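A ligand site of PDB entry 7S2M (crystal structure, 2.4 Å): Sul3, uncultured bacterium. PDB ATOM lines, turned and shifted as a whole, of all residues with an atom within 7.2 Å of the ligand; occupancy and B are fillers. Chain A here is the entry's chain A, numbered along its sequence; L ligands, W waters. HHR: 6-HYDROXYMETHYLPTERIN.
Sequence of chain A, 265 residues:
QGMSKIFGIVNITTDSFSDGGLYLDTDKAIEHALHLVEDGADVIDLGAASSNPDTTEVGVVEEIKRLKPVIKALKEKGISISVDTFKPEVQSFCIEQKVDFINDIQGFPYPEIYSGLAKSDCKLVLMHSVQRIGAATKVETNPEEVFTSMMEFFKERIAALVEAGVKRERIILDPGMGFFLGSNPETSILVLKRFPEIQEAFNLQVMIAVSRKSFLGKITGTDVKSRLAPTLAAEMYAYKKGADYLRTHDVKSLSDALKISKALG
A nitrogen (N2) of the ligand is in hydrogen-bond range of the side-chain amide oxygen (OD1) of Asn 103, 2.7 Å away. A nitrogen (N8) of the ligand lies within hydrogen-bond range of the side-chain carboxylate (OD2) of Asp 84. The side-chain amino group (NZ) of Lys 213 is in hydrogen-bond range of an oxygen (O4) of the ligand (2.9 Å). N3 of the ligand is in hydrogen-bond range of SD of Met 127, at 3.2 Å. The guanidinium group (NH2) of Arg 247 lies close to a nitrogen (N8) of the ligand, at 3.3 Å. The side-chain carboxylate (OD2) of Asp 174 is in hydrogen-bond range of a nitrogen (N3) of the ligand.
Merely in contact with the ligand: Phe 180 (3.4 Å), Ala 209 (3.5 Å), Ile 105 (3.6 Å), Met 207 (3.9 Å) and Val 125 (3.9 Å). Hydrophobic or aromatic side chains that line the ligand: Ile 105, Val 125, Met 127, Phe 180, Met 207 and Ala 209. Within 4 Å of the ligand: Asp 84, Asn 103, Ile 105, Val 125, Met 127, Asp 174, Phe 180, Met 207, Ala 209, Lys 213 and Arg 247. The nearest printed residue that does not touch the ligand is Met 177 (4.7 Å).
OD2 of Asp 45 lies within hydrogen-bond range of ND2 of Asn 103 (3.1 Å). OD2 of Asp 84 lies within salt-bridge range of NH1 of Arg 247 (2.9 Å). The guanidinium group (NE) of Arg 247 lies within salt-bridge range of the side-chain carboxylate (OD2) of Asp 45, at 3.7 Å. O of Ile 208 lies within hydrogen-bond range of N of Arg 247 (3.2 Å). The side-chain carboxylate of Asp 174 lies within hydrogen-bond range of the backbone NH of Gly 176. The backbone NH (N) of Asp 174 lies within hydrogen-bond range of the backbone carbonyl oxygen (O) of Leu 126 (2.6 Å).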
ATOM      1  N   PHE A   7      21.899 -34.138  -8.375  1.00  0.00           N
ATOM      2  CA  PHE A   7      22.403 -32.838  -8.801  1.00  0.00           C
ATOM      3  C   PHE A   7      23.657 -32.497  -8.015  1.00  0.00           C
ATOM      4  O   PHE A   7      23.604 -32.339  -6.788  1.00  0.00           O
ATOM      5  CB  PHE A   7      21.334 -31.754  -8.598  1.00  0.00           C
ATOM      6  CG  PHE A   7      20.521 -31.460  -9.820  1.00  0.00           C
ATOM      7  CD1 PHE A   7      19.956 -32.482 -10.570  1.00  0.00           C
ATOM      8  CD2 PHE A   7      20.318 -30.151 -10.240  1.00  0.00           C
ATOM      9  CE1 PHE A   7      19.209 -32.210 -11.701  1.00  0.00           C
ATOM     10  CE2 PHE A   7      19.575 -29.866 -11.366  1.00  0.00           C
ATOM     11  CZ  PHE A   7      19.018 -30.908 -12.094  1.00  0.00           C
ATOM     12  N   ILE A   9      26.212 -29.988  -6.722  1.00  0.00           N
ATOM     13  CA  ILE A   9      26.243 -28.550  -6.483  1.00  0.00           C
ATOM     14  C   ILE A   9      27.667 -28.042  -6.693  1.00  0.00           C
ATOM     15  O   ILE A   9      28.617 -28.548  -6.101  1.00  0.00           O
ATOM     16  CB  ILE A   9      25.744 -28.226  -5.065  1.00  0.00           C
ATOM     17  CG1 ILE A   9      24.249 -28.533  -4.946  1.00  0.00           C
ATOM     18  CG2 ILE A   9      26.008 -26.757  -4.725  1.00  0.00           C
ATOM     19  CD1 ILE A   9      23.732 -28.527  -3.524  1.00  0.00           C
ATOM     20  N   ASP A  45      24.951 -28.711 -10.958  1.00  0.00           N
ATOM     21  CA  ASP A  45      24.155 -27.526 -10.666  1.00  0.00           C
ATOM     22  C   ASP A  45      25.104 -26.360 -10.427  1.00  0.00           C
ATOM     23  O   ASP A  45      25.607 -26.157  -9.318  1.00  0.00           O
ATOM     24  CB  ASP A  45      23.237 -27.761  -9.466  1.00  0.00           C
ATOM     25  CG  ASP A  45      22.114 -26.736  -9.389  1.00  0.00           C
ATOM     26  OD1 ASP A  45      21.775 -26.140 -10.435  1.00  0.00           O
ATOM     27  OD2 ASP A  45      21.558 -26.551  -8.283  1.00  0.00           O
ATOM     28  N   ASP A  84      21.968 -22.447 -11.570  1.00  0.00           N
ATOM     29  CA  ASP A  84      21.218 -22.006 -10.386  1.00  0.00           C
ATOM     30  C   ASP A  84      21.202 -20.481 -10.407  1.00  0.00           C
ATOM     31  O   ASP A  84      22.078 -19.826  -9.839  1.00  0.00           O
ATOM     32  CB  ASP A  84      21.854 -22.562  -9.120  1.00  0.00           C
ATOM     33  CG  ASP A  84      20.995 -22.348  -7.888  1.00  0.00           C
ATOM     34  OD1 ASP A  84      20.028 -21.557  -7.946  1.00  0.00           O
ATOM     35  OD2 ASP A  84      21.282 -22.984  -6.852  1.00  0.00           O
ATOM     36  N   ASN A 103      17.688 -23.733 -13.040  1.00  0.00           N
ATOM     37  CA  ASN A 103      17.220 -23.867 -11.659  1.00  0.00           C
ATOM     38  C   ASN A 103      16.898 -22.479 -11.122  1.00  0.00           C
ATOM     39  O   ASN A 103      17.798 -21.675 -10.858  1.00  0.00           O
ATOM     40  CB  ASN A 103      18.267 -24.561 -10.807  1.00  0.00           C
ATOM     41  CG  ASN A 103      17.806 -24.801  -9.389  1.00  0.00           C
ATOM     42  OD1 ASN A 103      16.635 -24.628  -9.067  1.00  0.00           O
ATOM     43  ND2 ASN A 103      18.725 -25.223  -8.526  1.00  0.00           N
ATOM     44  N   ASP A 104      15.613 -22.194 -10.951  1.00  0.00           N
ATOM     45  CA  ASP A 104      15.133 -20.907 -10.450  1.00  0.00           C
ATOM     46  C   ASP A 104      14.534 -21.113  -9.065  1.00  0.00           C
ATOM     47  O   ASP A 104      13.547 -21.849  -8.918  1.00  0.00           O
ATOM     48  CB  ASP A 104      14.096 -20.303 -11.395  1.00  0.00           C
ATOM     49  CG  ASP A 104      13.799 -18.843 -11.088  1.00  0.00           C
ATOM     50  OD1 ASP A 104      14.072 -18.385  -9.963  1.00  0.00           O
ATOM     51  OD2 ASP A 104      13.287 -18.147 -11.989  1.00  0.00           O
ATOM     52  N   ILE A 105      15.119 -20.469  -8.050  1.00  0.00           N
ATOM     53  CA  ILE A 105      14.604 -20.567  -6.694  1.00  0.00           C
ATOM     54  C   ILE A 105      13.468 -19.596  -6.423  1.00  0.00           C
ATOM     55  O   ILE A 105      12.945 -19.560  -5.300  1.00  0.00           O
ATOM     56  CB  ILE A 105      15.726 -20.329  -5.656  1.00  0.00           C
ATOM     57  CG1 ILE A 105      16.372 -18.960  -5.880  1.00  0.00           C
ATOM     58  CG2 ILE A 105      16.767 -21.428  -5.729  1.00  0.00           C
ATOM     59  CD1 ILE A 105      16.687 -18.225  -4.599  1.00  0.00           C
ATOM     60  N   VAL A 125      13.278 -26.037 -13.253  1.00  0.00           N
ATOM     61  CA  VAL A 125      13.130 -26.446 -11.863  1.00  0.00           C
ATOM     62  C   VAL A 125      12.331 -25.376 -11.128  1.00  0.00           C
ATOM     63  O   VAL A 125      12.893 -24.388 -10.643  1.00  0.00           O
ATOM     64  CB  VAL A 125      14.489 -26.682 -11.197  1.00  0.00           C
ATOM     65  CG1 VAL A 125      14.308 -27.254  -9.790  1.00  0.00           C
ATOM     66  CG2 VAL A 125      15.344 -27.609 -12.045  1.00  0.00           C
ATOM     67  N   LEU A 126      11.018 -25.547 -11.065  1.00  0.00           N
ATOM     68  CA  LEU A 126      10.142 -24.588 -10.422  1.00  0.00           C
ATOM     69  C   LEU A 126      10.170 -24.806  -8.912  1.00  0.00           C
ATOM     70  O   LEU A 126       9.779 -25.873  -8.431  1.00  0.00           O
ATOM     71  CB  LEU A 126       8.719 -24.725 -10.960  1.00  0.00           C
ATOM     72  CG  LEU A 126       7.847 -23.469 -11.023  1.00  0.00           C
ATOM     73  CD1 LEU A 126       6.687 -23.693 -11.976  1.00  0.00           C
ATOM     74  CD2 LEU A 126       7.336 -23.074  -9.652  1.00  0.00           C
ATOM     75  N   MET A 127      10.643 -23.808  -8.175  1.00  0.00           N
ATOM     76  CA  MET A 127      10.757 -23.885  -6.720  1.00  0.00           C
ATOM     77  C   MET A 127       9.722 -22.987  -6.050  1.00  0.00           C
ATOM     78  O   MET A 127       9.406 -21.911  -6.547  1.00  0.00           O
ATOM     79  CB  MET A 127      12.157 -23.487  -6.249  1.00  0.00           C
ATOM     80  CG  MET A 127      12.628 -24.264  -5.037  1.00  0.00           C
ATOM     81  SD  MET A 127      14.185 -23.663  -4.373  1.00  0.00           S
ATOM     82  CE  MET A 127      13.730 -23.377  -2.674  1.00  0.00           C
ATOM     83  N   ASP A 174       9.990 -28.215  -7.253  1.00  0.00           N
ATOM     84  CA  ASP A 174      10.728 -28.249  -5.999  1.00  0.00           C
ATOM     85  C   ASP A 174       9.897 -27.558  -4.921  1.00  0.00           C
ATOM     86  O   ASP A 174       9.539 -26.381  -5.093  1.00  0.00           O
ATOM     87  CB  ASP A 174      12.101 -27.571  -6.139  1.00  0.00           C
ATOM     88  CG  ASP A 174      13.006 -27.817  -4.943  1.00  0.00           C
ATOM     89  OD1 ASP A 174      12.581 -27.563  -3.797  1.00  0.00           O
ATOM     90  OD2 ASP A 174      14.151 -28.272  -5.158  1.00  0.00           O
ATOM     91  N   PRO A 175       9.550 -28.235  -3.824  1.00  0.00           N
ATOM     92  CA  PRO A 175       8.685 -27.607  -2.820  1.00  0.00           C
ATOM     93  C   PRO A 175       9.390 -26.613  -1.912  1.00  0.00           C
ATOM     94  O   PRO A 175       8.708 -25.939  -1.128  1.00  0.00           O
ATOM     95  CB  PRO A 175       8.176 -28.817  -2.020  1.00  0.00           C
ATOM     96  CG  PRO A 175       9.289 -29.803  -2.104  1.00  0.00           C
ATOM     97  CD  PRO A 175       9.894 -29.627  -3.481  1.00  0.00           C
ATOM     98  N   GLY A 176      10.707 -26.504  -1.985  1.00  0.00           N
ATOM     99  CA  GLY A 176      11.444 -25.670  -1.051  1.00  0.00           C
ATOM    100  C   GLY A 176      11.738 -26.410   0.222  1.00  0.00           C
ATOM    101  O   GLY A 176      11.002 -27.326   0.601  1.00  0.00           O
ATOM    102  N   MET A 177      12.821 -26.045   0.912  1.00  0.00           N
ATOM    103  CA  MET A 177      13.226 -26.761   2.118  1.00  0.00           C
ATOM    104  C   MET A 177      13.871 -25.813   3.102  1.00  0.00           C
ATOM    105  O   MET A 177      14.588 -24.883   2.706  1.00  0.00           O
ATOM    106  CB  MET A 177      14.199 -27.897   1.772  1.00  0.00           C
ATOM    107  CG  MET A 177      13.555 -29.173   1.256  1.00  0.00           C
ATOM    108  SD  MET A 177      12.323 -29.940   2.336  1.00  0.00           S
ATOM    109  CE  MET A 177      13.063 -29.741   3.943  1.00  0.00           C
ATOM    110  N   GLY A 178      13.634 -26.049   4.386  1.00  0.00           N
ATOM    111  CA  GLY A 178      14.293 -25.313   5.444  1.00  0.00           C
ATOM    112  C   GLY A 178      13.882 -23.857   5.542  1.00  0.00           C
ATOM    113  O   GLY A 178      12.705 -23.542   5.735  1.00  0.00           O
ATOM    114  N   PHE A 180      13.589 -21.731   3.297  1.00  0.00           N
ATOM    115  CA  PHE A 180      12.652 -21.352   2.249  1.00  0.00           C
ATOM    116  C   PHE A 180      11.205 -21.608   2.647  1.00  0.00           C
ATOM    117  O   PHE A 180      10.300 -21.071   1.992  1.00  0.00           O
ATOM    118  CB  PHE A 180      12.981 -22.109   0.953  1.00  0.00           C
ATOM    119  CG  PHE A 180      14.244 -21.645   0.292  1.00  0.00           C
ATOM    120  CD1 PHE A 180      14.312 -20.397  -0.308  1.00  0.00           C
ATOM    121  CD2 PHE A 180      15.363 -22.459   0.259  1.00  0.00           C
ATOM    122  CE1 PHE A 180      15.480 -19.971  -0.919  1.00  0.00           C
ATOM    123  CE2 PHE A 180      16.534 -22.043  -0.353  1.00  0.00           C
ATOM    124  CZ  PHE A 180      16.582 -20.792  -0.940  1.00  0.00           C
ATOM    125  N   MET A 207      11.888 -32.540  -7.126  1.00  0.00           N
ATOM    126  CA  MET A 207      13.264 -32.484  -6.648  1.00  0.00           C
ATOM    127  C   MET A 207      13.276 -32.118  -5.168  1.00  0.00           C
ATOM    128  O   MET A 207      12.566 -31.194  -4.747  1.00  0.00           O
ATOM    129  CB  MET A 207      14.081 -31.467  -7.450  1.00  0.00           C
ATOM    130  CG  MET A 207      15.557 -31.444  -7.067  1.00  0.00           C
ATOM    131  SD  MET A 207      16.376 -29.904  -7.535  1.00  0.00           S
ATOM    132  CE  MET A 207      16.870 -30.305  -9.206  1.00  0.00           C
ATOM    133  N   ILE A 208      14.083 -32.825  -4.393  1.00  0.00           N
ATOM    134  CA  ILE A 208      14.269 -32.562  -2.968  1.00  0.00           C
ATOM    135  C   ILE A 208      15.690 -32.071  -2.758  1.00  0.00           C
ATOM    136  O   ILE A 208      16.654 -32.681  -3.244  1.00  0.00           O
ATOM    137  CB  ILE A 208      13.975 -33.809  -2.123  1.00  0.00           C
ATOM    138  CG1 ILE A 208      12.521 -34.239  -2.291  1.00  0.00           C
ATOM    139  CG2 ILE A 208      14.288 -33.543  -0.651  1.00  0.00           C
ATOM    140  CD1 ILE A 208      11.524 -33.340  -1.580  1.00  0.00           C
ATOM    141  N   ALA A 209      15.830 -30.953  -2.035  1.00  0.00           N
ATOM    142  CA  ALA A 209      17.132 -30.350  -1.743  1.00  0.00           C
ATOM    143  C   ALA A 209      17.202 -30.060  -0.253  1.00  0.00           C
ATOM    144  O   ALA A 209      16.715 -29.020   0.204  1.00  0.00           O
ATOM    145  CB  ALA A 209      17.353 -29.089  -2.573  1.00  0.00           C
ATOM    146  N   VAL A 210      17.805 -30.972   0.509  1.00  0.00           N
ATOM    147  CA  VAL A 210      17.960 -30.819   1.953  1.00  0.00           C
ATOM    148  C   VAL A 210      19.411 -30.720   2.374  1.00  0.00           C
ATOM    149  O   VAL A 210      19.686 -30.619   3.582  1.00  0.00           O
ATOM    150  CB  VAL A 210      17.277 -31.975   2.708  1.00  0.00           C
ATOM    151  CG1 VAL A 210      15.764 -31.811   2.673  1.00  0.00           C
ATOM    152  CG2 VAL A 210      17.700 -33.312   2.126  1.00  0.00           C
ATOM    153  N   SER A 211      20.352 -30.733   1.434  1.00  0.00           N
ATOM    154  CA  SER A 211      21.764 -30.818   1.764  1.00  0.00           C
ATOM    155  C   SER A 211      22.217 -29.605   2.571  1.00  0.00           C
ATOM    156  O   SER A 211      22.187 -28.473   2.080  1.00  0.00           O
ATOM    157  CB  SER A 211      22.599 -30.944   0.495  1.00  0.00           C
ATOM    158  OG  SER A 211      23.973 -31.095   0.783  1.00  0.00           O
ATOM    159  N   ARG A 212      22.620 -29.852   3.819  1.00  0.00           N
ATOM    160  CA  ARG A 212      23.203 -28.839   4.699  1.00  0.00           C
ATOM    161  C   ARG A 212      22.259 -27.643   4.881  1.00  0.00           C
ATOM    162  O   ARG A 212      22.569 -26.513   4.488  1.00  0.00           O
ATOM    163  CB  ARG A 212      24.577 -28.392   4.174  1.00  0.00           C
ATOM    164  CG  ARG A 212      25.421 -29.504   3.584  1.00  0.00           C
ATOM    165  CD  ARG A 212      26.824 -29.527   4.181  1.00  0.00           C
ATOM    166  NE  ARG A 212      27.710 -30.437   3.463  1.00  0.00           N
ATOM    167  CZ  ARG A 212      28.726 -30.042   2.709  1.00  0.00           C
ATOM    168  NH1 ARG A 212      29.016 -28.769   2.549  1.00  0.00           N
ATOM    169  NH2 ARG A 212      29.457 -30.960   2.087  1.00  0.00           N
ATOM    170  N   LYS A 213      21.116 -27.919   5.479  1.00  0.00           N
ATOM    171  CA  LYS A 213      20.132 -26.893   5.809  1.00  0.00           C
ATOM    172  C   LYS A 213      19.978 -26.806   7.322  1.00  0.00           C
ATOM    173  O   LYS A 213      20.109 -27.811   8.030  1.00  0.00           O
ATOM    174  CB  LYS A 213      18.784 -27.177   5.139  1.00  0.00           C
ATOM    175  CG  LYS A 213      18.895 -27.388   3.636  1.00  0.00           C
ATOM    176  CD  LYS A 213      18.081 -26.363   2.857  1.00  0.00           C
ATOM    177  CE  LYS A 213      18.371 -26.463   1.369  1.00  0.00           C
ATOM    178  NZ  LYS A 213      17.672 -25.414   0.581  1.00  0.00           N
ATOM    179  N   ARG A 247      19.333 -32.739  -4.994  1.00  0.00           N
ATOM    180  CA  ARG A 247      20.388 -31.727  -4.985  1.00  0.00           C
ATOM    181  C   ARG A 247      21.212 -31.911  -3.723  1.00  0.00           C
ATOM    182  O   ARG A 247      20.684 -31.812  -2.611  1.00  0.00           O
ATOM    183  CB  ARG A 247      19.791 -30.324  -5.061  1.00  0.00           C
ATOM    184  CG  ARG A 247      20.554 -29.367  -5.967  1.00  0.00           C
ATOM    185  CD  ARG A 247      20.027 -27.946  -5.828  1.00  0.00           C
ATOM    186  NE  ARG A 247      20.661 -27.232  -4.731  1.00  0.00           N
ATOM    187  CZ  ARG A 247      21.454 -26.185  -4.878  1.00  0.00           C
ATOM    188  NH1 ARG A 247      21.736 -25.690  -6.065  1.00  0.00           N
ATOM    189  NH2 ARG A 247      21.982 -25.618  -3.793  1.00  0.00           N
ATOM    190  N   HIS A 249      25.480 -31.834  -1.831  1.00  0.00           N
ATOM    191  CA  HIS A 249      26.879 -31.398  -1.833  1.00  0.00           C
ATOM    192  C   HIS A 249      27.830 -32.575  -1.885  1.00  0.00           C
ATOM    193  O   HIS A 249      28.647 -32.689  -2.813  1.00  0.00           O
ATOM    194  CB  HIS A 249      27.159 -30.546  -0.587  1.00  0.00           C
ATOM    195  CG  HIS A 249      26.577 -29.170  -0.650  1.00  0.00           C
ATOM    196  ND1 HIS A 249      25.886 -28.595   0.399  1.00  0.00           N
ATOM    197  CD2 HIS A 249      26.597 -28.235  -1.641  1.00  0.00           C
ATOM    198  CE1 HIS A 249      25.508 -27.377   0.059  1.00  0.00           C
ATOM    199  NE2 HIS A 249      25.918 -27.142  -1.170  1.00  0.00           N
HETATM  200  C7  HHR L   1      20.106 -22.918  -3.481  1.00  0.00           C
HETATM  201  N8  HHR L   1      19.564 -23.448  -4.564  1.00  0.00           N
HETATM  202  C9  HHR L   1      18.512 -24.291  -4.469  1.00  0.00           C
HETATM  203  N1  HHR L   1      17.957 -24.825  -5.571  1.00  0.00           N
HETATM  204  C2  HHR L   1      16.893 -25.674  -5.471  1.00  0.00           C
HETATM  205  N2  HHR L   1      16.474 -26.115  -6.782  1.00  0.00           N
HETATM  206  C10 HHR L   1      18.003 -24.596  -3.255  1.00  0.00           C
HETATM  207  C4  HHR L   1      16.922 -25.462  -3.155  1.00  0.00           C
HETATM  208  N3  HHR L   1      16.380 -25.980  -4.247  1.00  0.00           N
HETATM  209  O4  HHR L   1      16.458 -25.744  -2.062  1.00  0.00           O
HETATM  210  N5  HHR L   1      18.571 -24.058  -2.136  1.00  0.00           N
HETATM  211  C6  HHR L   1      19.585 -23.240  -2.231  1.00  0.00           C
HETATM  212  C6A HHR L   1      20.102 -22.720  -0.870  1.00  0.00           C
HETATM  213  O6A HHR L   1      20.831 -23.785  -0.195  1.00  0.00           O
HETATM  214  O   HOH W   1      22.981 -24.971  -0.399  1.00  0.00           O
